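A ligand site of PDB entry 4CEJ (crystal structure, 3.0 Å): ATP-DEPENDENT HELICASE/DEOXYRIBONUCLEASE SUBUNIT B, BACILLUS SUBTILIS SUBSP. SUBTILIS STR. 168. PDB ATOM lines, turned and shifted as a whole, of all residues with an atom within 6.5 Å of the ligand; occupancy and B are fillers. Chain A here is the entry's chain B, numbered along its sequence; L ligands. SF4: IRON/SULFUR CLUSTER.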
ATOM      1  N   ALA A 800      24.357  10.811   1.850  1.00  0.00           N
ATOM      2  CA  ALA A 800      23.053  10.168   1.974  1.00  0.00           C
ATOM      3  C   ALA A 800      22.694  10.036   3.447  1.00  0.00           C
ATOM      4  O   ALA A 800      21.554  10.289   3.844  1.00  0.00           O
ATOM      5  CB  ALA A 800      23.070   8.814   1.294  1.00  0.00           C
ATOM      6  N   CYS A 801      23.687   9.646   4.234  1.00  0.00           N
ATOM      7  CA  CYS A 801      23.546   9.454   5.666  1.00  0.00           C
ATOM      8  C   CYS A 801      24.921   9.209   6.276  1.00  0.00           C
ATOM      9  O   CYS A 801      25.607   8.264   5.904  1.00  0.00           O
ATOM     10  CB  CYS A 801      22.610   8.279   5.971  1.00  0.00           C
ATOM     11  SG  CYS A 801      22.599   7.734   7.687  1.00  0.00           S
ATOM     12  N   PRO A 802      25.335  10.079   7.211  1.00  0.00           N
ATOM     13  CA  PRO A 802      26.652   9.930   7.839  1.00  0.00           C
ATOM     14  C   PRO A 802      26.824   8.564   8.523  1.00  0.00           C
ATOM     15  O   PRO A 802      27.871   7.944   8.370  1.00  0.00           O
ATOM     16  CB  PRO A 802      26.687  11.063   8.879  1.00  0.00           C
ATOM     17  CG  PRO A 802      25.764  12.091   8.308  1.00  0.00           C
ATOM     18  CD  PRO A 802      24.659  11.321   7.644  1.00  0.00           C
ATOM     19  N   PHE A 803      25.793   8.113   9.242  1.00  0.00           N
ATOM     20  CA  PHE A 803      25.904   6.861   9.981  1.00  0.00           C
ATOM     21  C   PHE A 803      26.105   5.666   9.051  1.00  0.00           C
ATOM     22  O   PHE A 803      26.827   4.734   9.381  1.00  0.00           O
ATOM     23  CB  PHE A 803      24.667   6.633  10.851  1.00  0.00           C
ATOM     24  CG  PHE A 803      24.789   5.438  11.765  1.00  0.00           C
ATOM     25  CD1 PHE A 803      25.314   5.576  13.030  1.00  0.00           C
ATOM     26  CD2 PHE A 803      24.373   4.179  11.346  1.00  0.00           C
ATOM     27  CE1 PHE A 803      25.433   4.477  13.870  1.00  0.00           C
ATOM     28  CE2 PHE A 803      24.482   3.092  12.177  1.00  0.00           C
ATOM     29  CZ  PHE A 803      25.019   3.238  13.439  1.00  0.00           C
ATOM     30  N   SER A 804      25.445   5.696   7.901  1.00  0.00           N
ATOM     31  CA  SER A 804      25.596   4.618   6.928  1.00  0.00           C
ATOM     32  C   SER A 804      27.049   4.554   6.490  1.00  0.00           C
ATOM     33  O   SER A 804      27.622   3.469   6.359  1.00  0.00           O
ATOM     34  CB  SER A 804      24.667   4.833   5.732  1.00  0.00           C
ATOM     35  OG  SER A 804      24.986   6.027   5.058  1.00  0.00           O
ATOM     36  N   HIS A 805      27.650   5.718   6.268  1.00  0.00           N
ATOM     37  CA  HIS A 805      29.058   5.804   5.904  1.00  0.00           C
ATOM     38  C   HIS A 805      29.943   5.324   7.062  1.00  0.00           C
ATOM     39  O   HIS A 805      31.039   4.827   6.836  1.00  0.00           O
ATOM     40  CB  HIS A 805      29.423   7.233   5.510  1.00  0.00           C
ATOM     41  CG  HIS A 805      30.902   7.472   5.419  1.00  0.00           C
ATOM     42  ND1 HIS A 805      31.665   7.834   6.516  1.00  0.00           N
ATOM     43  CD2 HIS A 805      31.763   7.404   4.382  1.00  0.00           C
ATOM     44  CE1 HIS A 805      32.918   7.973   6.149  1.00  0.00           C
ATOM     45  NE2 HIS A 805      33.009   7.722   4.860  1.00  0.00           N
ATOM     46  N   SER A1109      26.345  10.933  12.449  1.00  0.00           N
ATOM     47  CA  SER A1109      24.949  11.094  12.852  1.00  0.00           C
ATOM     48  C   SER A1109      23.962  10.435  11.888  1.00  0.00           C
ATOM     49  O   SER A1109      24.189  10.389  10.687  1.00  0.00           O
ATOM     50  CB  SER A1109      24.612  12.581  12.981  1.00  0.00           C
ATOM     51  OG  SER A1109      24.928  13.272  11.787  1.00  0.00           O
ATOM     52  N   ILE A1110      22.863   9.941  12.443  1.00  0.00           N
ATOM     53  CA  ILE A1110      21.818   9.275  11.658  1.00  0.00           C
ATOM     54  C   ILE A1110      20.891  10.297  11.017  1.00  0.00           C
ATOM     55  O   ILE A1110      19.924  10.740  11.624  1.00  0.00           O
ATOM     56  CB  ILE A1110      21.000   8.309  12.529  1.00  0.00           C
ATOM     57  CG1 ILE A1110      21.917   7.311  13.236  1.00  0.00           C
ATOM     58  CG2 ILE A1110      19.957   7.570  11.692  1.00  0.00           C
ATOM     59  CD1 ILE A1110      21.188   6.298  14.099  1.00  0.00           C
ATOM     60  N   GLU A1111      21.196  10.672   9.773  1.00  0.00           N
ATOM     61  CA  GLU A1111      20.442  11.702   9.081  1.00  0.00           C
ATOM     62  C   GLU A1111      19.979  11.257   7.700  1.00  0.00           C
ATOM     63  O   GLU A1111      20.535  11.693   6.687  1.00  0.00           O
ATOM     64  CB  GLU A1111      21.288  12.968   8.946  1.00  0.00           C
ATOM     65  CG  GLU A1111      21.665  13.617  10.268  1.00  0.00           C
ATOM     66  CD  GLU A1111      22.705  14.688  10.089  1.00  0.00           C
ATOM     67  OE1 GLU A1111      22.898  15.163   8.948  1.00  0.00           O
ATOM     68  OE2 GLU A1111      23.360  15.051  11.089  1.00  0.00           O
ATOM     69  N   PRO A1112      18.960  10.401   7.638  1.00  0.00           N
ATOM     70  CA  PRO A1112      18.404   9.914   6.369  1.00  0.00           C
ATOM     71  C   PRO A1112      17.651  11.023   5.643  1.00  0.00           C
ATOM     72  O   PRO A1112      16.885  11.746   6.278  1.00  0.00           O
ATOM     73  CB  PRO A1112      17.450   8.789   6.781  1.00  0.00           C
ATOM     74  CG  PRO A1112      17.640   8.610   8.274  1.00  0.00           C
ATOM     75  CD  PRO A1112      18.183   9.890   8.790  1.00  0.00           C
ATOM     76  N   THR A1119      13.950   7.364  -0.030  1.00  0.00           N
ATOM     77  CA  THR A1119      14.894   7.397   1.079  1.00  0.00           C
ATOM     78  C   THR A1119      16.028   6.389   0.880  1.00  0.00           C
ATOM     79  O   THR A1119      15.820   5.346   0.248  1.00  0.00           O
ATOM     80  CB  THR A1119      14.184   7.127   2.419  1.00  0.00           C
ATOM     81  OG1 THR A1119      13.693   5.776   2.436  1.00  0.00           O
ATOM     82  CG2 THR A1119      13.024   8.083   2.621  1.00  0.00           C
ATOM     83  N   PRO A1120      17.221   6.689   1.413  1.00  0.00           N
ATOM     84  CA  PRO A1120      18.358   5.763   1.353  1.00  0.00           C
ATOM     85  C   PRO A1120      18.058   4.449   2.065  1.00  0.00           C
ATOM     86  O   PRO A1120      18.561   3.399   1.682  1.00  0.00           O
ATOM     87  CB  PRO A1120      19.489   6.516   2.080  1.00  0.00           C
ATOM     88  CG  PRO A1120      19.050   7.922   2.134  1.00  0.00           C
ATOM     89  CD  PRO A1120      17.572   7.970   2.068  1.00  0.00           C
ATOM     90  N   CYS A1121      17.232   4.544   3.110  1.00  0.00           N
ATOM     91  CA  CYS A1121      17.014   3.452   4.070  1.00  0.00           C
ATOM     92  C   CYS A1121      16.622   2.119   3.425  1.00  0.00           C
ATOM     93  O   CYS A1121      17.072   1.061   3.862  1.00  0.00           O
ATOM     94  CB  CYS A1121      15.951   3.852   5.089  1.00  0.00           C
ATOM     95  SG  CYS A1121      16.347   5.387   5.959  1.00  0.00           S
ATOM     96  N   THR A1122      15.798   2.189   2.390  1.00  0.00           N
ATOM     97  CA  THR A1122      15.351   0.980   1.707  1.00  0.00           C
ATOM     98  C   THR A1122      16.514   0.218   1.084  1.00  0.00           C
ATOM     99  O   THR A1122      16.527  -1.014   1.090  1.00  0.00           O
ATOM    100  CB  THR A1122      14.319   1.294   0.601  1.00  0.00           C
ATOM    101  OG1 THR A1122      14.380   2.686   0.272  1.00  0.00           O
ATOM    102  CG2 THR A1122      12.919   0.946   1.080  1.00  0.00           C
ATOM    103  N   CYS A1124      19.596   0.256   2.097  1.00  0.00           N
ATOM    104  CA  CYS A1124      20.683   0.235   3.071  1.00  0.00           C
ATOM    105  C   CYS A1124      20.602  -0.971   4.009  1.00  0.00           C
ATOM    106  O   CYS A1124      19.544  -1.279   4.558  1.00  0.00           O
ATOM    107  CB  CYS A1124      20.698   1.531   3.880  1.00  0.00           C
ATOM    108  SG  CYS A1124      22.065   1.689   5.051  1.00  0.00           S
ATOM    109  N   ALA A1125      21.730  -1.634   4.212  1.00  0.00           N
ATOM    110  CA  ALA A1125      21.781  -2.874   4.985  1.00  0.00           C
ATOM    111  C   ALA A1125      21.884  -2.650   6.496  1.00  0.00           C
ATOM    112  O   ALA A1125      21.757  -3.585   7.282  1.00  0.00           O
ATOM    113  CB  ALA A1125      22.938  -3.735   4.511  1.00  0.00           C
ATOM    114  N   PHE A1126      22.124  -1.404   6.896  1.00  0.00           N
ATOM    115  CA  PHE A1126      22.418  -1.113   8.302  1.00  0.00           C
ATOM    116  C   PHE A1126      21.222  -0.591   9.076  1.00  0.00           C
ATOM    117  O   PHE A1126      21.381   0.057  10.107  1.00  0.00           O
ATOM    118  CB  PHE A1126      23.569  -0.104   8.400  1.00  0.00           C
ATOM    119  CG  PHE A1126      24.753  -0.448   7.553  1.00  0.00           C
ATOM    120  CD1 PHE A1126      25.514  -1.574   7.840  1.00  0.00           C
ATOM    121  CD2 PHE A1126      25.111   0.335   6.469  1.00  0.00           C
ATOM    122  CE1 PHE A1126      26.611  -1.889   7.066  1.00  0.00           C
ATOM    123  CE2 PHE A1126      26.211   0.025   5.688  1.00  0.00           C
ATOM    124  CZ  PHE A1126      26.964  -1.098   5.987  1.00  0.00           C
ATOM    125  N   LYS A1127      20.016  -0.895   8.587  1.00  0.00           N
ATOM    126  CA  LYS A1127      18.790  -0.412   9.230  1.00  0.00           C
ATOM    127  C   LYS A1127      18.657  -0.939  10.646  1.00  0.00           C
ATOM    128  O   LYS A1127      18.104  -0.265  11.520  1.00  0.00           O
ATOM    129  CB  LYS A1127      17.569  -0.813   8.390  1.00  0.00           C
ATOM    130  CG  LYS A1127      16.248  -0.256   8.902  1.00  0.00           C
ATOM    131  CD  LYS A1127      15.562   0.619   7.866  1.00  0.00           C
ATOM    132  CE  LYS A1127      14.873  -0.199   6.773  1.00  0.00           C
ATOM    133  NZ  LYS A1127      15.800  -0.679   5.716  1.00  0.00           N
ATOM    134  N   SER A1128      19.182  -2.137  10.897  1.00  0.00           N
ATOM    135  CA  SER A1128      19.086  -2.737  12.225  1.00  0.00           C
ATOM    136  C   SER A1128      20.183  -2.248  13.153  1.00  0.00           C
ATOM    137  O   SER A1128      20.090  -2.431  14.365  1.00  0.00           O
ATOM    138  CB  SER A1128      19.143  -4.262  12.118  1.00  0.00           C
ATOM    139  OG  SER A1128      20.387  -4.700  11.606  1.00  0.00           O
ATOM    140  N   VAL A1129      21.222  -1.635  12.592  1.00  0.00           N
ATOM    141  CA  VAL A1129      22.299  -1.081  13.389  1.00  0.00           C
ATOM    142  C   VAL A1129      21.925   0.314  13.893  1.00  0.00           C
ATOM    143  O   VAL A1129      22.080   0.633  15.063  1.00  0.00           O
ATOM    144  CB  VAL A1129      23.621  -1.003  12.617  1.00  0.00           C
ATOM    145  CG1 VAL A1129      24.751  -0.580  13.538  1.00  0.00           C
ATOM    146  CG2 VAL A1129      23.926  -2.341  11.968  1.00  0.00           C
ATOM    147  N   CYS A1130      21.432   1.140  12.971  1.00  0.00           N
ATOM    148  CA  CYS A1130      21.022   2.496  13.313  1.00  0.00           C
ATOM    149  C   CYS A1130      19.829   2.490  14.258  1.00  0.00           C
ATOM    150  O   CYS A1130      19.744   3.313  15.166  1.00  0.00           O
ATOM    151  CB  CYS A1130      20.673   3.277  12.056  1.00  0.00           C
ATOM    152  SG  CYS A1130      19.149   2.726  11.264  1.00  0.00           S
ATOM    153  N   GLN A1131      18.905   1.568  14.006  1.00  0.00           N
ATOM    154  CA  GLN A1131      17.686   1.447  14.804  1.00  0.00           C
ATOM    155  C   GLN A1131      16.900   2.748  14.764  1.00  0.00           C
ATOM    156  O   GLN A1131      16.313   3.172  15.756  1.00  0.00           O
ATOM    157  CB  GLN A1131      18.026   1.044  16.239  1.00  0.00           C
ATOM    158  CG  GLN A1131      18.697  -0.314  16.294  1.00  0.00           C
ATOM    159  CD  GLN A1131      19.571  -0.493  17.507  1.00  0.00           C
ATOM    160  OE1 GLN A1131      19.327   0.072  18.565  1.00  0.00           O
ATOM    161  NE2 GLN A1131      20.617  -1.298  17.351  1.00  0.00           N
ATOM    162  N   PHE A1132      16.918   3.359  13.580  1.00  0.00           N
ATOM    163  CA  PHE A1132      16.160   4.573  13.293  1.00  0.00           C
ATOM    164  C   PHE A1132      14.687   4.411  13.639  1.00  0.00           C
ATOM    165  O   PHE A1132      14.052   3.429  13.272  1.00  0.00           O
ATOM    166  CB  PHE A1132      16.344   4.947  11.814  1.00  0.00           C
ATOM    167  CG  PHE A1132      15.694   6.236  11.418  1.00  0.00           C
ATOM    168  CD1 PHE A1132      16.360   7.440  11.566  1.00  0.00           C
ATOM    169  CD2 PHE A1132      14.425   6.239  10.888  1.00  0.00           C
ATOM    170  CE1 PHE A1132      15.753   8.642  11.192  1.00  0.00           C
ATOM    171  CE2 PHE A1132      13.814   7.431  10.505  1.00  0.00           C
ATOM    172  CZ  PHE A1132      14.481   8.622  10.656  1.00  0.00           C
ATOM    173  N   TYR A1141      13.678  12.320   9.280  1.00  0.00           N
ATOM    174  CA  TYR A1141      14.198  12.400   7.917  1.00  0.00           C
ATOM    175  C   TYR A1141      14.586  13.834   7.563  1.00  0.00           C
ATOM    176  O   TYR A1141      13.967  14.785   8.021  1.00  0.00           O
ATOM    177  CB  TYR A1141      13.152  11.874   6.919  1.00  0.00           C
ATOM    178  CG  TYR A1141      12.899  10.389   6.994  1.00  0.00           C
ATOM    179  CD1 TYR A1141      11.959   9.863   7.868  1.00  0.00           C
ATOM    180  CD2 TYR A1141      13.604   9.504   6.191  1.00  0.00           C
ATOM    181  CE1 TYR A1141      11.726   8.503   7.938  1.00  0.00           C
ATOM    182  CE2 TYR A1141      13.383   8.138   6.261  1.00  0.00           C
ATOM    183  CZ  TYR A1141      12.438   7.647   7.132  1.00  0.00           C
ATOM    184  OH  TYR A1141      12.204   6.287   7.201  1.00  0.00           O
HETATM  185 FE1  SF4 L   1      21.047   6.042   7.759  1.00  0.00          FE
HETATM  186 FE2  SF4 L   1      18.427   4.718   6.724  1.00  0.00          FE
HETATM  187 FE3  SF4 L   1      19.861   3.584   9.252  1.00  0.00          FE
HETATM  188 FE4  SF4 L   1      21.127   3.243   6.458  1.00  0.00          FE
HETATM  189  S1  SF4 L   1      19.181   2.763   7.337  1.00  0.00           S
HETATM  190  S2  SF4 L   1      21.806   4.078   8.369  1.00  0.00           S
HETATM  191  S3  SF4 L   1      20.381   5.201   5.850  1.00  0.00           S
HETATM  192  S4  SF4 L   1      19.094   5.546   8.638  1.00  0.00           S
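The side-chain sulfur (SG) of Cys 1124 binds an iron atom (FE4) of the ligand.
The side-chain sulfur (SG) of Cys 801 is bound to an iron atom (FE1) of the ligand, at 2.3 Å.
An iron atom (FE2) of the ligand is bound by the side-chain sulfur (SG) of Cys 1121, 2.3 Å away.
FE3 of the ligand is bound by SG of Cys 1130 (2.3 Å).
The backbone NH (N) of Phe 1126 lies close to the side-chain sulfur (SG) of Cys 1124 (3.6 Å).
The backbone carbonyl oxygen (O) of Ser 1109 is in hydrogen-bond range of the backbone NH (N) of Phe 803 (3.1 Å).
SG of Cys 1130 sits close to O of Lys 1127 (3.2 Å).
OG of Ser 804 sits at hydrogen-bond distance from O of Cys 801, 2.5 Å away.
The backbone NH of Phe 803 sits close to the side-chain sulfur of Cys 801, at 3.6 Å.
The backbone carbonyl oxygen (O) of Cys 1121 lies within hydrogen-bond range of the side-chain amino group (NZ) of Lys 1127 (2.8 Å).
N of Phe 1132 lies close to SG of Cys 1130 (3.3 Å).
SG of Cys 1130 sits close to O of Phe 1126 (3.7 Å).
Merely in contact with the ligand: Pro 1112 (3.4 Å), Lys 1127 (3.7 Å), Ile 1110 (3.8 Å), Phe 803 (3.9 Å), Phe 1126 (3.9 Å) and Ser 804 (3.9 Å).
Hydrophobic or aromatic side chains within 4 Å of the ligand: Phe 803, Ile 1110 and Pro 1112.
Of the 24 residues printed, 10 come within 4 Å of the ligand.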
